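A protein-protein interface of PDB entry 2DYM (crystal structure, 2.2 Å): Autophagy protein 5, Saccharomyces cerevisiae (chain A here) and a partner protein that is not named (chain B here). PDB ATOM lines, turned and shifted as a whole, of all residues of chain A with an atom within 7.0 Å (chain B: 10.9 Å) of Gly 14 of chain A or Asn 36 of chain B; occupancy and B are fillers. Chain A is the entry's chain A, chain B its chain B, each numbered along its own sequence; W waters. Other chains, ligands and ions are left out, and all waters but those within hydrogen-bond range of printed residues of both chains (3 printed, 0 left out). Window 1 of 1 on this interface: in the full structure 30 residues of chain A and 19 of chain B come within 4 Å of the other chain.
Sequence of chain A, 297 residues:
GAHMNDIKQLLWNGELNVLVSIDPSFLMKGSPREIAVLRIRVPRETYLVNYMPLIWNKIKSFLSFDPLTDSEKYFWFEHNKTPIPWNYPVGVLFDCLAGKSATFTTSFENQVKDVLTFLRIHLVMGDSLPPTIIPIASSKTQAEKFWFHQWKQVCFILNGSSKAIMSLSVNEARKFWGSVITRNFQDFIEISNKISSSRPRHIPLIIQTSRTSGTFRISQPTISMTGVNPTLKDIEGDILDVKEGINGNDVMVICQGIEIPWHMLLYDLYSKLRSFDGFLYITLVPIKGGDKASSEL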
ATOM      1  N   LYS A   8      16.376   0.940  -5.688  1.00  0.00           N
ATOM      2  CA  LYS A   8      15.303   1.323  -6.601  1.00  0.00           C
ATOM      3  C   LYS A   8      15.795   1.572  -8.028  1.00  0.00           C
ATOM      4  O   LYS A   8      15.093   1.263  -8.990  1.00  0.00           O
ATOM      5  CB  LYS A   8      14.557   2.555  -6.065  1.00  0.00           C
ATOM      6  CG  LYS A   8      13.656   2.231  -4.865  1.00  0.00           C
ATOM      7  CD  LYS A   8      12.820   3.430  -4.420  1.00  0.00           C
ATOM      8  CE  LYS A   8      11.904   3.052  -3.246  1.00  0.00           C
ATOM      9  NZ  LYS A   8      11.093   4.215  -2.778  1.00  0.00           N
ATOM     10  N   GLN A   9      16.995   2.132  -8.160  1.00  0.00           N
ATOM     11  CA  GLN A   9      17.587   2.392  -9.476  1.00  0.00           C
ATOM     12  C   GLN A   9      17.839   1.044 -10.174  1.00  0.00           C
ATOM     13  O   GLN A   9      17.532   0.870 -11.352  1.00  0.00           O
ATOM     14  CB  GLN A   9      18.910   3.157  -9.310  1.00  0.00           C
ATOM     15  CG  GLN A   9      19.647   3.466 -10.613  1.00  0.00           C
ATOM     16  CD  GLN A   9      18.881   4.423 -11.508  1.00  0.00           C
ATOM     17  OE1 GLN A   9      18.270   4.019 -12.505  1.00  0.00           O
ATOM     18  NE2 GLN A   9      18.901   5.699 -11.150  1.00  0.00           N
ATOM     19  N   LEU A  10      18.371   0.090  -9.421  1.00  0.00           N
ATOM     20  CA  LEU A  10      18.652  -1.245  -9.935  1.00  0.00           C
ATOM     21  C   LEU A  10      17.358  -1.919 -10.424  1.00  0.00           C
ATOM     22  O   LEU A  10      17.373  -2.646 -11.421  1.00  0.00           O
ATOM     23  CB  LEU A  10      19.299  -2.086  -8.834  1.00  0.00           C
ATOM     24  CG  LEU A  10      20.799  -2.447  -8.807  1.00  0.00           C
ATOM     25  CD1 LEU A  10      21.612  -1.705  -9.870  1.00  0.00           C
ATOM     26  CD2 LEU A  10      21.324  -2.181  -7.406  1.00  0.00           C
ATOM     27  N   LEU A  11      16.247  -1.679  -9.719  1.00  0.00           N
ATOM     28  CA  LEU A  11      14.951  -2.244 -10.101  1.00  0.00           C
ATOM     29  C   LEU A  11      14.434  -1.565 -11.362  1.00  0.00           C
ATOM     30  O   LEU A  11      13.858  -2.218 -12.244  1.00  0.00           O
ATOM     31  CB  LEU A  11      13.914  -2.056  -8.984  1.00  0.00           C
ATOM     32  CG  LEU A  11      14.144  -2.813  -7.673  1.00  0.00           C
ATOM     33  CD1 LEU A  11      13.016  -2.495  -6.695  1.00  0.00           C
ATOM     34  CD2 LEU A  11      14.212  -4.310  -7.953  1.00  0.00           C
ATOM     35  N   TRP A  12      14.639  -0.254 -11.439  1.00  0.00           N
ATOM     36  CA  TRP A  12      14.195   0.528 -12.589  1.00  0.00           C
ATOM     37  C   TRP A  12      14.961   0.104 -13.834  1.00  0.00           C
ATOM     38  O   TRP A  12      14.429   0.150 -14.953  1.00  0.00           O
ATOM     39  CB  TRP A  12      14.440   2.010 -12.331  1.00  0.00           C
ATOM     40  CG  TRP A  12      13.707   2.909 -13.265  1.00  0.00           C
ATOM     41  CD1 TRP A  12      14.239   3.648 -14.288  1.00  0.00           C
ATOM     42  CD2 TRP A  12      12.304   3.206 -13.241  1.00  0.00           C
ATOM     43  NE1 TRP A  12      13.253   4.391 -14.896  1.00  0.00           N
ATOM     44  CE2 TRP A  12      12.058   4.139 -14.272  1.00  0.00           C
ATOM     45  CE3 TRP A  12      11.233   2.777 -12.442  1.00  0.00           C
ATOM     46  CZ2 TRP A  12      10.779   4.655 -14.528  1.00  0.00           C
ATOM     47  CZ3 TRP A  12       9.961   3.291 -12.698  1.00  0.00           C
ATOM     48  CH2 TRP A  12       9.748   4.220 -13.733  1.00  0.00           C
ATOM     49  N   ASN A  13      16.217  -0.293 -13.623  1.00  0.00           N
ATOM     50  CA  ASN A  13      17.090  -0.740 -14.703  1.00  0.00           C
ATOM     51  C   ASN A  13      16.744  -2.173 -15.131  1.00  0.00           C
ATOM     52  O   ASN A  13      17.201  -2.632 -16.184  1.00  0.00           O
ATOM     53  CB  ASN A  13      18.561  -0.694 -14.256  1.00  0.00           C
ATOM     54  CG  ASN A  13      19.088   0.727 -14.086  1.00  0.00           C
ATOM     55  OD1 ASN A  13      20.161   0.941 -13.515  1.00  0.00           O
ATOM     56  ND2 ASN A  13      18.346   1.694 -14.593  1.00  0.00           N
ATOM     57  N   GLY A  14      15.952  -2.872 -14.314  1.00  0.00           N
ATOM     58  CA  GLY A  14      15.567  -4.239 -14.642  1.00  0.00           C
ATOM     59  C   GLY A  14      15.075  -4.341 -16.075  1.00  0.00           C
ATOM     60  O   GLY A  14      14.208  -3.572 -16.488  1.00  0.00           O
ATOM     61  N   GLU A  15      15.626  -5.279 -16.838  1.00  0.00           N
ATOM     62  CA  GLU A  15      15.241  -5.439 -18.243  1.00  0.00           C
ATOM     63  C   GLU A  15      15.381  -6.892 -18.681  1.00  0.00           C
ATOM     64  O   GLU A  15      16.335  -7.565 -18.318  1.00  0.00           O
ATOM     65  CB  GLU A  15      16.111  -4.534 -19.129  1.00  0.00           C
ATOM     66  CG  GLU A  15      15.517  -4.208 -20.494  1.00  0.00           C
ATOM     67  CD  GLU A  15      16.359  -3.179 -21.241  1.00  0.00           C
ATOM     68  OE1 GLU A  15      17.455  -3.531 -21.737  1.00  0.00           O
ATOM     69  OE2 GLU A  15      15.931  -2.010 -21.317  1.00  0.00           O
ATOM     70  N   LEU A  16      14.437  -7.355 -19.490  1.00  0.00           N
ATOM     71  CA  LEU A  16      14.421  -8.743 -19.941  1.00  0.00           C
ATOM     72  C   LEU A  16      14.446  -8.950 -21.446  1.00  0.00           C
ATOM     73  O   LEU A  16      13.916  -8.136 -22.207  1.00  0.00           O
ATOM     74  CB  LEU A  16      13.161  -9.437 -19.410  1.00  0.00           C
ATOM     75  CG  LEU A  16      12.940  -9.580 -17.902  1.00  0.00           C
ATOM     76  CD1 LEU A  16      11.511 -10.080 -17.634  1.00  0.00           C
ATOM     77  CD2 LEU A  16      13.964 -10.555 -17.332  1.00  0.00           C
ATOM     78  N   ARG A  41      13.540  -5.969 -25.998  1.00  0.00           N
ATOM     79  CA  ARG A  41      13.952  -5.795 -24.614  1.00  0.00           C
ATOM     80  C   ARG A  41      12.776  -5.109 -23.929  1.00  0.00           C
ATOM     81  O   ARG A  41      12.223  -4.144 -24.450  1.00  0.00           O
ATOM     82  CB  ARG A  41      15.196  -4.913 -24.526  1.00  0.00           C
ATOM     83  CG  ARG A  41      16.477  -5.580 -25.026  1.00  0.00           C
ATOM     84  CD  ARG A  41      16.997  -6.611 -24.038  1.00  0.00           C
ATOM     85  NE  ARG A  41      17.657  -5.999 -22.885  1.00  0.00           N
ATOM     86  CZ  ARG A  41      18.056  -6.668 -21.802  1.00  0.00           C
ATOM     87  NH1 ARG A  41      17.870  -7.981 -21.704  1.00  0.00           N
ATOM     88  NH2 ARG A  41      18.641  -6.019 -20.810  1.00  0.00           N
ATOM     89  N   VAL A  42      12.375  -5.624 -22.775  1.00  0.00           N
ATOM     90  CA  VAL A  42      11.262  -5.042 -22.045  1.00  0.00           C
ATOM     91  C   VAL A  42      11.630  -4.890 -20.572  1.00  0.00           C
ATOM     92  O   VAL A  42      12.124  -5.828 -19.949  1.00  0.00           O
ATOM     93  CB  VAL A  42      10.005  -5.935 -22.155  1.00  0.00           C
ATOM     94  CG1 VAL A  42       8.839  -5.313 -21.378  1.00  0.00           C
ATOM     95  CG2 VAL A  42       9.629  -6.120 -23.610  1.00  0.00           C
ATOM     96  N   PRO A  43      11.434  -3.692 -20.003  1.00  0.00           N
ATOM     97  CA  PRO A  43      11.782  -3.562 -18.582  1.00  0.00           C
ATOM     98  C   PRO A  43      10.862  -4.399 -17.693  1.00  0.00           C
ATOM     99  O   PRO A  43       9.739  -4.733 -18.075  1.00  0.00           O
ATOM    100  CB  PRO A  43      11.641  -2.056 -18.307  1.00  0.00           C
ATOM    101  CG  PRO A  43      10.806  -1.526 -19.445  1.00  0.00           C
ATOM    102  CD  PRO A  43      11.195  -2.376 -20.627  1.00  0.00           C
ATOM    103  N   ARG A  44      11.355  -4.757 -16.513  1.00  0.00           N
ATOM    104  CA  ARG A  44      10.559  -5.525 -15.563  1.00  0.00           C
ATOM    105  C   ARG A  44       9.421  -4.663 -15.009  1.00  0.00           C
ATOM    106  O   ARG A  44       8.296  -5.139 -14.805  1.00  0.00           O
ATOM    107  CB  ARG A  44      11.440  -5.997 -14.395  1.00  0.00           C
ATOM    108  CG  ARG A  44      12.229  -7.272 -14.667  1.00  0.00           C
ATOM    109  CD  ARG A  44      13.207  -7.561 -13.552  1.00  0.00           C
ATOM    110  NE  ARG A  44      13.637  -8.956 -13.551  1.00  0.00           N
ATOM    111  CZ  ARG A  44      12.981  -9.936 -12.929  1.00  0.00           C
ATOM    112  NH1 ARG A  44      13.437 -11.179 -12.986  1.00  0.00           N
ATOM    113  NH2 ARG A  44      11.887  -9.668 -12.219  1.00  0.00           N
ATOM    114  N   GLU A  45       9.729  -3.390 -14.776  1.00  0.00           N
ATOM    115  CA  GLU A  45       8.778  -2.446 -14.198  1.00  0.00           C
ATOM    116  C   GLU A  45       7.929  -1.721 -15.233  1.00  0.00           C
ATOM    117  O   GLU A  45       8.109  -0.522 -15.460  1.00  0.00           O
ATOM    118  CB  GLU A  45       9.527  -1.414 -13.341  1.00  0.00           C
ATOM    119  CG  GLU A  45      10.310  -1.995 -12.171  1.00  0.00           C
ATOM    120  CD  GLU A  45       9.419  -2.647 -11.108  1.00  0.00           C
ATOM    121  OE1 GLU A  45       9.942  -2.959 -10.010  1.00  0.00           O
ATOM    122  OE2 GLU A  45       8.207  -2.852 -11.366  1.00  0.00           O
ATOM    123  N   ARG A 183      10.593   6.078 -18.883  1.00  0.00           N
ATOM    124  CA  ARG A 183      11.655   5.565 -18.028  1.00  0.00           C
ATOM    125  C   ARG A 183      12.348   6.665 -17.220  1.00  0.00           C
ATOM    126  O   ARG A 183      13.517   6.523 -16.845  1.00  0.00           O
ATOM    127  CB  ARG A 183      12.695   4.827 -18.873  1.00  0.00           C
ATOM    128  CG  ARG A 183      12.154   3.653 -19.685  1.00  0.00           C
ATOM    129  CD  ARG A 183      12.049   2.415 -18.811  1.00  0.00           C
ATOM    130  NE  ARG A 183      10.771   2.333 -18.135  1.00  0.00           N
ATOM    131  CZ  ARG A 183      10.538   1.636 -17.025  1.00  0.00           C
ATOM    132  NH1 ARG A 183      11.502   0.954 -16.429  1.00  0.00           N
ATOM    133  NH2 ARG A 183       9.316   1.600 -16.519  1.00  0.00           N
ATOM    134  N   GLN A 256      11.202  -9.653  -6.848  1.00  0.00           N
ATOM    135  CA  GLN A 256      12.009  -8.915  -7.821  1.00  0.00           C
ATOM    136  C   GLN A 256      13.103  -9.804  -8.433  1.00  0.00           C
ATOM    137  O   GLN A 256      14.249  -9.385  -8.597  1.00  0.00           O
ATOM    138  CB  GLN A 256      12.634  -7.680  -7.162  1.00  0.00           C
ATOM    139  CG  GLN A 256      11.630  -6.571  -6.828  1.00  0.00           C
ATOM    140  CD  GLN A 256      11.123  -5.833  -8.065  1.00  0.00           C
ATOM    141  OE1 GLN A 256      11.563  -6.089  -9.185  1.00  0.00           O
ATOM    142  NE2 GLN A 256      10.199  -4.903  -7.858  1.00  0.00           N
ATOM    143  N   ILE A 258      14.742 -12.187  -7.173  1.00  0.00           N
ATOM    144  CA  ILE A 258      15.811 -12.656  -6.301  1.00  0.00           C
ATOM    145  C   ILE A 258      15.278 -13.342  -5.054  1.00  0.00           C
ATOM    146  O   ILE A 258      14.102 -13.208  -4.690  1.00  0.00           O
ATOM    147  CB  ILE A 258      16.754 -11.514  -5.835  1.00  0.00           C
ATOM    148  CG1 ILE A 258      15.979 -10.511  -4.981  1.00  0.00           C
ATOM    149  CG2 ILE A 258      17.421 -10.859  -7.043  1.00  0.00           C
ATOM    150  CD1 ILE A 258      16.849  -9.453  -4.322  1.00  0.00           C
ATOM    151  N   LEU B  27      23.409  -7.071   0.494  1.00  0.00           N
ATOM    152  CA  LEU B  27      22.969  -8.355  -0.031  1.00  0.00           C
ATOM    153  C   LEU B  27      21.987  -8.121  -1.191  1.00  0.00           C
ATOM    154  O   LEU B  27      22.108  -8.740  -2.252  1.00  0.00           O
ATOM    155  CB  LEU B  27      22.293  -9.156   1.085  1.00  0.00           C
ATOM    156  CG  LEU B  27      21.715 -10.537   0.779  1.00  0.00           C
ATOM    157  CD1 LEU B  27      22.809 -11.455   0.273  1.00  0.00           C
ATOM    158  CD2 LEU B  27      21.091 -11.105   2.041  1.00  0.00           C
ATOM    159  N   LEU B  28      21.023  -7.221  -0.989  1.00  0.00           N
ATOM    160  CA  LEU B  28      20.042  -6.909  -2.031  1.00  0.00           C
ATOM    161  C   LEU B  28      20.746  -6.273  -3.238  1.00  0.00           C
ATOM    162  O   LEU B  28      20.488  -6.651  -4.382  1.00  0.00           O
ATOM    163  CB  LEU B  28      18.967  -5.947  -1.494  1.00  0.00           C
ATOM    164  CG  LEU B  28      18.112  -6.428  -0.314  1.00  0.00           C
ATOM    165  CD1 LEU B  28      17.166  -5.321   0.128  1.00  0.00           C
ATOM    166  CD2 LEU B  28      17.332  -7.665  -0.711  1.00  0.00           C
ATOM    167  N   ILE B  29      21.633  -5.312  -2.985  1.00  0.00           N
ATOM    168  CA  ILE B  29      22.357  -4.641  -4.065  1.00  0.00           C
ATOM    169  C   ILE B  29      23.098  -5.683  -4.908  1.00  0.00           C
ATOM    170  O   ILE B  29      23.050  -5.684  -6.139  1.00  0.00           O
ATOM    171  CB  ILE B  29      23.392  -3.635  -3.507  1.00  0.00           C
ATOM    172  CG1 ILE B  29      22.675  -2.519  -2.741  1.00  0.00           C
ATOM    173  CG2 ILE B  29      24.226  -3.063  -4.649  1.00  0.00           C
ATOM    174  CD1 ILE B  29      21.834  -1.614  -3.597  1.00  0.00           C
ATOM    175  N   ARG B  30      23.794  -6.571  -4.220  1.00  0.00           N
ATOM    176  CA  ARG B  30      24.553  -7.606  -4.883  1.00  0.00           C
ATOM    177  C   ARG B  30      23.651  -8.514  -5.717  1.00  0.00           C
ATOM    178  O   ARG B  30      23.930  -8.767  -6.900  1.00  0.00           O
ATOM    179  CB  ARG B  30      25.280  -8.451  -3.851  1.00  0.00           C
ATOM    180  CG  ARG B  30      26.218  -9.428  -4.487  1.00  0.00           C
ATOM    181  CD  ARG B  30      27.373  -8.686  -5.134  1.00  0.00           C
ATOM    182  NE  ARG B  30      28.028  -9.534  -6.113  1.00  0.00           N
ATOM    183  CZ  ARG B  30      27.635  -9.659  -7.375  1.00  0.00           C
ATOM    184  NH1 ARG B  30      26.593  -8.975  -7.826  1.00  0.00           N
ATOM    185  NH2 ARG B  30      28.266 -10.499  -8.182  1.00  0.00           N
ATOM    186  N   ARG B  31      22.572  -9.003  -5.110  1.00  0.00           N
ATOM    187  CA  ARG B  31      21.674  -9.909  -5.814  1.00  0.00           C
ATOM    188  C   ARG B  31      20.956  -9.277  -7.004  1.00  0.00           C
ATOM    189  O   ARG B  31      20.748  -9.941  -8.017  1.00  0.00           O
ATOM    190  CB  ARG B  31      20.669 -10.513  -4.830  1.00  0.00           C
ATOM    191  CG  ARG B  31      21.330 -11.501  -3.871  1.00  0.00           C
ATOM    192  CD  ARG B  31      20.356 -12.107  -2.864  1.00  0.00           C
ATOM    193  NE  ARG B  31      20.978 -13.222  -2.156  1.00  0.00           N
ATOM    194  CZ  ARG B  31      20.407 -13.918  -1.175  1.00  0.00           C
ATOM    195  NH1 ARG B  31      19.180 -13.625  -0.762  1.00  0.00           N
ATOM    196  NH2 ARG B  31      21.072 -14.913  -0.603  1.00  0.00           N
ATOM    197  N   LEU B  32      20.594  -7.997  -6.889  1.00  0.00           N
ATOM    198  CA  LEU B  32      19.891  -7.292  -7.970  1.00  0.00           C
ATOM    199  C   LEU B  32      20.855  -7.036  -9.138  1.00  0.00           C
ATOM    200  O   LEU B  32      20.464  -7.122 -10.307  1.00  0.00           O
ATOM    201  CB  LEU B  32      19.331  -5.959  -7.468  1.00  0.00           C
ATOM    202  CG  LEU B  32      17.863  -5.814  -7.092  1.00  0.00           C
ATOM    203  CD1 LEU B  32      17.131  -7.146  -7.060  1.00  0.00           C
ATOM    204  CD2 LEU B  32      17.774  -5.057  -5.770  1.00  0.00           C
ATOM    205  N   THR B  33      22.107  -6.710  -8.826  1.00  0.00           N
ATOM    206  CA  THR B  33      23.102  -6.462  -9.860  1.00  0.00           C
ATOM    207  C   THR B  33      23.323  -7.753 -10.646  1.00  0.00           C
ATOM    208  O   THR B  33      23.395  -7.750 -11.874  1.00  0.00           O
ATOM    209  CB  THR B  33      24.445  -6.002  -9.218  1.00  0.00           C
ATOM    210  OG1 THR B  33      24.239  -4.787  -8.477  1.00  0.00           O
ATOM    211  CG2 THR B  33      25.496  -5.733 -10.293  1.00  0.00           C
ATOM    212  N   ASP B  34      23.444  -8.856  -9.923  1.00  0.00           N
ATOM    213  CA  ASP B  34      23.664 -10.150 -10.545  1.00  0.00           C
ATOM    214  C   ASP B  34      22.481 -10.479 -11.449  1.00  0.00           C
ATOM    215  O   ASP B  34      22.644 -10.932 -12.590  1.00  0.00           O
ATOM    216  CB  ASP B  34      23.811 -11.225  -9.474  1.00  0.00           C
ATOM    217  CG  ASP B  34      24.904 -12.220  -9.809  1.00  0.00           C
ATOM    218  OD1 ASP B  34      24.601 -13.431  -9.908  1.00  0.00           O
ATOM    219  OD2 ASP B  34      26.069 -11.783  -9.973  1.00  0.00           O
ATOM    220  N   ARG B  35      21.280 -10.243 -10.932  1.00  0.00           N
ATOM    221  CA  ARG B  35      20.062 -10.495 -11.686  1.00  0.00           C
ATOM    222  C   ARG B  35      20.111  -9.691 -12.978  1.00  0.00           C
ATOM    223  O   ARG B  35      19.917 -10.227 -14.065  1.00  0.00           O
ATOM    224  CB  ARG B  35      18.848 -10.069 -10.860  1.00  0.00           C
ATOM    225  CG  ARG B  35      17.521 -10.140 -11.590  1.00  0.00           C
ATOM    226  CD  ARG B  35      16.482  -9.276 -10.880  1.00  0.00           C
ATOM    227  NE  ARG B  35      16.572  -7.880 -11.306  1.00  0.00           N
ATOM    228  CZ  ARG B  35      15.642  -6.961 -11.058  1.00  0.00           C
ATOM    229  NH1 ARG B  35      15.809  -5.721 -11.502  1.00  0.00           N
ATOM    230  NH2 ARG B  35      14.549  -7.271 -10.352  1.00  0.00           N
ATOM    231  N   ASN B  36      20.372  -8.395 -12.863  1.00  0.00           N
ATOM    232  CA  ASN B  36      20.411  -7.561 -14.053  1.00  0.00           C
ATOM    233  C   ASN B  36      21.500  -8.034 -15.023  1.00  0.00           C
ATOM    234  O   ASN B  36      21.289  -8.039 -16.238  1.00  0.00           O
ATOM    235  CB  ASN B  36      20.595  -6.089 -13.672  1.00  0.00           C
ATOM    236  CG  ASN B  36      19.334  -5.483 -13.034  1.00  0.00           C
ATOM    237  OD1 ASN B  36      18.281  -6.122 -12.974  1.00  0.00           O
ATOM    238  ND2 ASN B  36      19.444  -4.242 -12.571  1.00  0.00           N
ATOM    239  N   ASP B  37      22.646  -8.450 -14.495  1.00  0.00           N
ATOM    240  CA  ASP B  37      23.717  -8.955 -15.352  1.00  0.00           C
ATOM    241  C   ASP B  37      23.255 -10.209 -16.109  1.00  0.00           C
ATOM    242  O   ASP B  37      23.415 -10.301 -17.328  1.00  0.00           O
ATOM    243  CB  ASP B  37      24.962  -9.269 -14.519  1.00  0.00           C
ATOM    244  CG  ASP B  37      25.726  -8.014 -14.116  1.00  0.00           C
ATOM    245  OD1 ASP B  37      26.618  -8.120 -13.248  1.00  0.00           O
ATOM    246  OD2 ASP B  37      25.437  -6.925 -14.668  1.00  0.00           O
ATOM    247  N   LYS B  38      22.670 -11.167 -15.396  1.00  0.00           N
ATOM    248  CA  LYS B  38      22.198 -12.384 -16.046  1.00  0.00           C
ATOM    249  C   LYS B  38      21.131 -12.077 -17.085  1.00  0.00           C
ATOM    250  O   LYS B  38      21.134 -12.640 -18.177  1.00  0.00           O
ATOM    251  CB  LYS B  38      21.605 -13.367 -15.027  1.00  0.00           C
ATOM    252  CG  LYS B  38      22.579 -13.853 -13.973  1.00  0.00           C
ATOM    253  CD  LYS B  38      21.985 -14.969 -13.119  1.00  0.00           C
ATOM    254  CE  LYS B  38      20.778 -14.499 -12.333  1.00  0.00           C
ATOM    255  NZ  LYS B  38      20.286 -15.565 -11.410  1.00  0.00           N
ATOM    256  N   GLU B  39      20.218 -11.176 -16.754  1.00  0.00           N
ATOM    257  CA  GLU B  39      19.139 -10.863 -17.669  1.00  0.00           C
ATOM    258  C   GLU B  39      19.578 -10.044 -18.880  1.00  0.00           C
ATOM    259  O   GLU B  39      18.930 -10.077 -19.927  1.00  0.00           O
ATOM    260  CB  GLU B  39      17.979 -10.209 -16.885  1.00  0.00           C
ATOM    261  CG  GLU B  39      17.281 -11.247 -15.967  1.00  0.00           C
ATOM    262  CD  GLU B  39      16.207 -10.703 -15.017  1.00  0.00           C
ATOM    263  OE1 GLU B  39      15.635 -11.528 -14.267  1.00  0.00           O
ATOM    264  OE2 GLU B  39      15.925  -9.484 -15.003  1.00  0.00           O
ATOM    265  N   ALA B  40      20.701  -9.348 -18.748  1.00  0.00           N
ATOM    266  CA  ALA B  40      21.242  -8.536 -19.840  1.00  0.00           C
ATOM    267  C   ALA B  40      22.147  -9.352 -20.781  1.00  0.00           C
ATOM    268  O   ALA B  40      22.368  -8.961 -21.936  1.00  0.00           O
ATOM    269  CB  ALA B  40      22.035  -7.362 -19.270  1.00  0.00           C
ATOM    270  N   HIS B  41      22.653 -10.487 -20.301  1.00  0.00           N
ATOM    271  CA  HIS B  41      23.554 -11.293 -21.117  1.00  0.00           C
ATOM    272  C   HIS B  41      22.969 -11.638 -22.483  1.00  0.00           C
ATOM    273  O   HIS B  41      21.826 -12.083 -22.589  1.00  0.00           O
ATOM    274  CB  HIS B  41      23.958 -12.572 -20.386  1.00  0.00           C
ATOM    275  CG  HIS B  41      25.072 -13.310 -21.062  1.00  0.00           C
ATOM    276  ND1 HIS B  41      26.307 -12.739 -21.291  1.00  0.00           N
ATOM    277  CD2 HIS B  41      25.123 -14.547 -21.610  1.00  0.00           C
ATOM    278  CE1 HIS B  41      27.067 -13.592 -21.955  1.00  0.00           C
ATOM    279  NE2 HIS B  41      26.372 -14.696 -22.160  1.00  0.00           N
ATOM    280  N   LEU B  42      23.762 -11.413 -23.526  1.00  0.00           N
ATOM    281  CA  LEU B  42      23.339 -11.677 -24.898  1.00  0.00           C
ATOM    282  C   LEU B  42      22.178 -10.773 -25.350  1.00  0.00           C
ATOM    283  O   LEU B  42      21.403 -11.138 -26.244  1.00  0.00           O
ATOM    284  CB  LEU B  42      22.960 -13.159 -25.055  1.00  0.00           C
ATOM    285  CG  LEU B  42      24.118 -14.153 -24.856  1.00  0.00           C
ATOM    286  CD1 LEU B  42      23.654 -15.585 -25.120  1.00  0.00           C
ATOM    287  CD2 LEU B  42      25.261 -13.792 -25.788  1.00  0.00           C
ATOM    288  N   ASN B  43      22.062  -9.591 -24.751  1.00  0.00           N
ATOM    289  CA  ASN B  43      20.994  -8.672 -25.131  1.00  0.00           C
ATOM    290  C   ASN B  43      21.153  -8.188 -26.586  1.00  0.00           C
ATOM    291  O   ASN B  43      20.205  -7.662 -27.184  1.00  0.00           O
ATOM    292  CB  ASN B  43      20.940  -7.466 -24.176  1.00  0.00           C
ATOM    293  CG  ASN B  43      22.155  -6.560 -24.303  1.00  0.00           C
ATOM    294  OD1 ASN B  43      23.211  -6.825 -23.725  1.00  0.00           O
ATOM    295  ND2 ASN B  43      22.013  -5.494 -25.079  1.00  0.00           N
HETATM  296  O   HOH W   1      17.015  -7.219 -15.322  1.00  0.00           O
HETATM  297  O   HOH W   2      19.016  -6.787 -17.930  1.00  0.00           O
HETATM  298  O   HOH W   3      12.871  -4.949 -11.406  1.00  0.00           O
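NH1 of Arg 35 of chain B lies within hydrogen-bond range of O of Leu 10 of chain A. The backbone carbonyl oxygen (O) of Leu 10 of chain A lies within hydrogen-bond range of the side-chain amide nitrogen (ND2) of Asn 36 of chain B. NH1 of Arg 41 of chain A is in hydrogen-bond range of O of Glu 39 of chain B (2.9 Å). The guanidinium group of Arg 44 of chain A is in salt-bridge range of the side-chain carboxylate of Glu 39 of chain B, at 2.6 Å. O of Gln 256 of chain A is in hydrogen-bond range of NH2 of Arg 35 of chain B (2.8 Å).
OE1 of Glu 15 of chain A lies within salt-bridge range of NE of Arg 41 of chain A, 2.7 Å away. The backbone carbonyl oxygen (O) of Ala 40 of chain B lies close to the side-chain amide oxygen (OD1) of Asn 43 of chain B, 2.9 Å away.
Among the printed residues, merely in contact across the chains: Leu 16 of chain A with Glu 39 of chain B, Glu 15 of chain A with Glu 39 of chain B, Gly 14 of chain A with Arg 35 of chain B, Arg 44 of chain A with Arg 35 of chain B, Ile 258 of chain A with Arg 31 of chain B, Ile 258 of chain A with Leu 32 of chain B, Gly 14 of chain A with Asn 36 of chain B, Arg 41 of chain A with Ala 40 of chain B, Arg 41 of chain A with Asn 43 of chain B, Leu 11 of chain A with Arg 35 of chain B, Leu 10 of chain A with Ile 29 of chain B and Gln 256 of chain A with Leu 32 of chain B.
Of chain B, only Ile 29 (3.9 Å), Arg 35 (3.5 Å) and Asn 36 (2.9 Å) come within 4 Å of Leu 10 of chain A. No residue of chain B comes within 4 Å of Asn 13 of chain A. Glu 15 of chain A touches just one residue of chain B: Glu 39 (3.4 Å). Of the printed residues of chain B, Leu 16 of chain A touches Glu 39 (3.2 Å). No residue of chain B comes within 4 Å of Pro 43 of chain A. Glu 45 of chain A touches none of the printed residues of chain B. Lys 38 of chain B touches none of the printed residues of chain A. The nearest residue of chain B that does not touch Gly 14 of chain A is Glu 39 of chain B (5.3 Å). The nearest printed residue of chain B that does not touch Leu 11 of chain A is Leu 32 of chain B (4.04 Å).
Of the 17 printed residues of chain A, 9 touch a printed residue of chain B. Printed residues of chain A that touch a printed residue of chain B: Leu 10, Leu 11, Gly 14, Glu 15, Leu 16, Arg 41, Arg 44, Gln 256 and Ile 258. Hydrophobic or aromatic side chains of chain A within 4 Å of the printed part of chain B: Leu 10, Leu 11, Leu 16 and Ile 258. Along chain A the printed residues that touch a printed residue of chain B span positions 10 to 258. Hydrophobic or aromatic side chains of chain B within 4 Å of the printed part of chain A: Ile 29, Leu 32 and Ala 40. Among the printed residues, 17 pairs touch across the chains. Among the printed residues, Asp or Glu carboxylates within 4 Å of a Lys or Arg side-chain nitrogen of the other chain: Arg 44 of chain A with Glu 39 of chain B (2.6 Å).
Water W1 lies within hydrogen-bond range of OE2 of Glu 39 of chain B (2.5 Å), N of Glu 15 of chain A (2.8 Å) and OD1 of Asn 36 of chain B (2.9 Å). Water W3 lies within hydrogen-bond range of OE1 of Gln 256 of chain A (2.8 Å), O of Leu 11 of chain A (3.0 Å) and NH1 of Arg 35 of chain B (3.0 Å).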
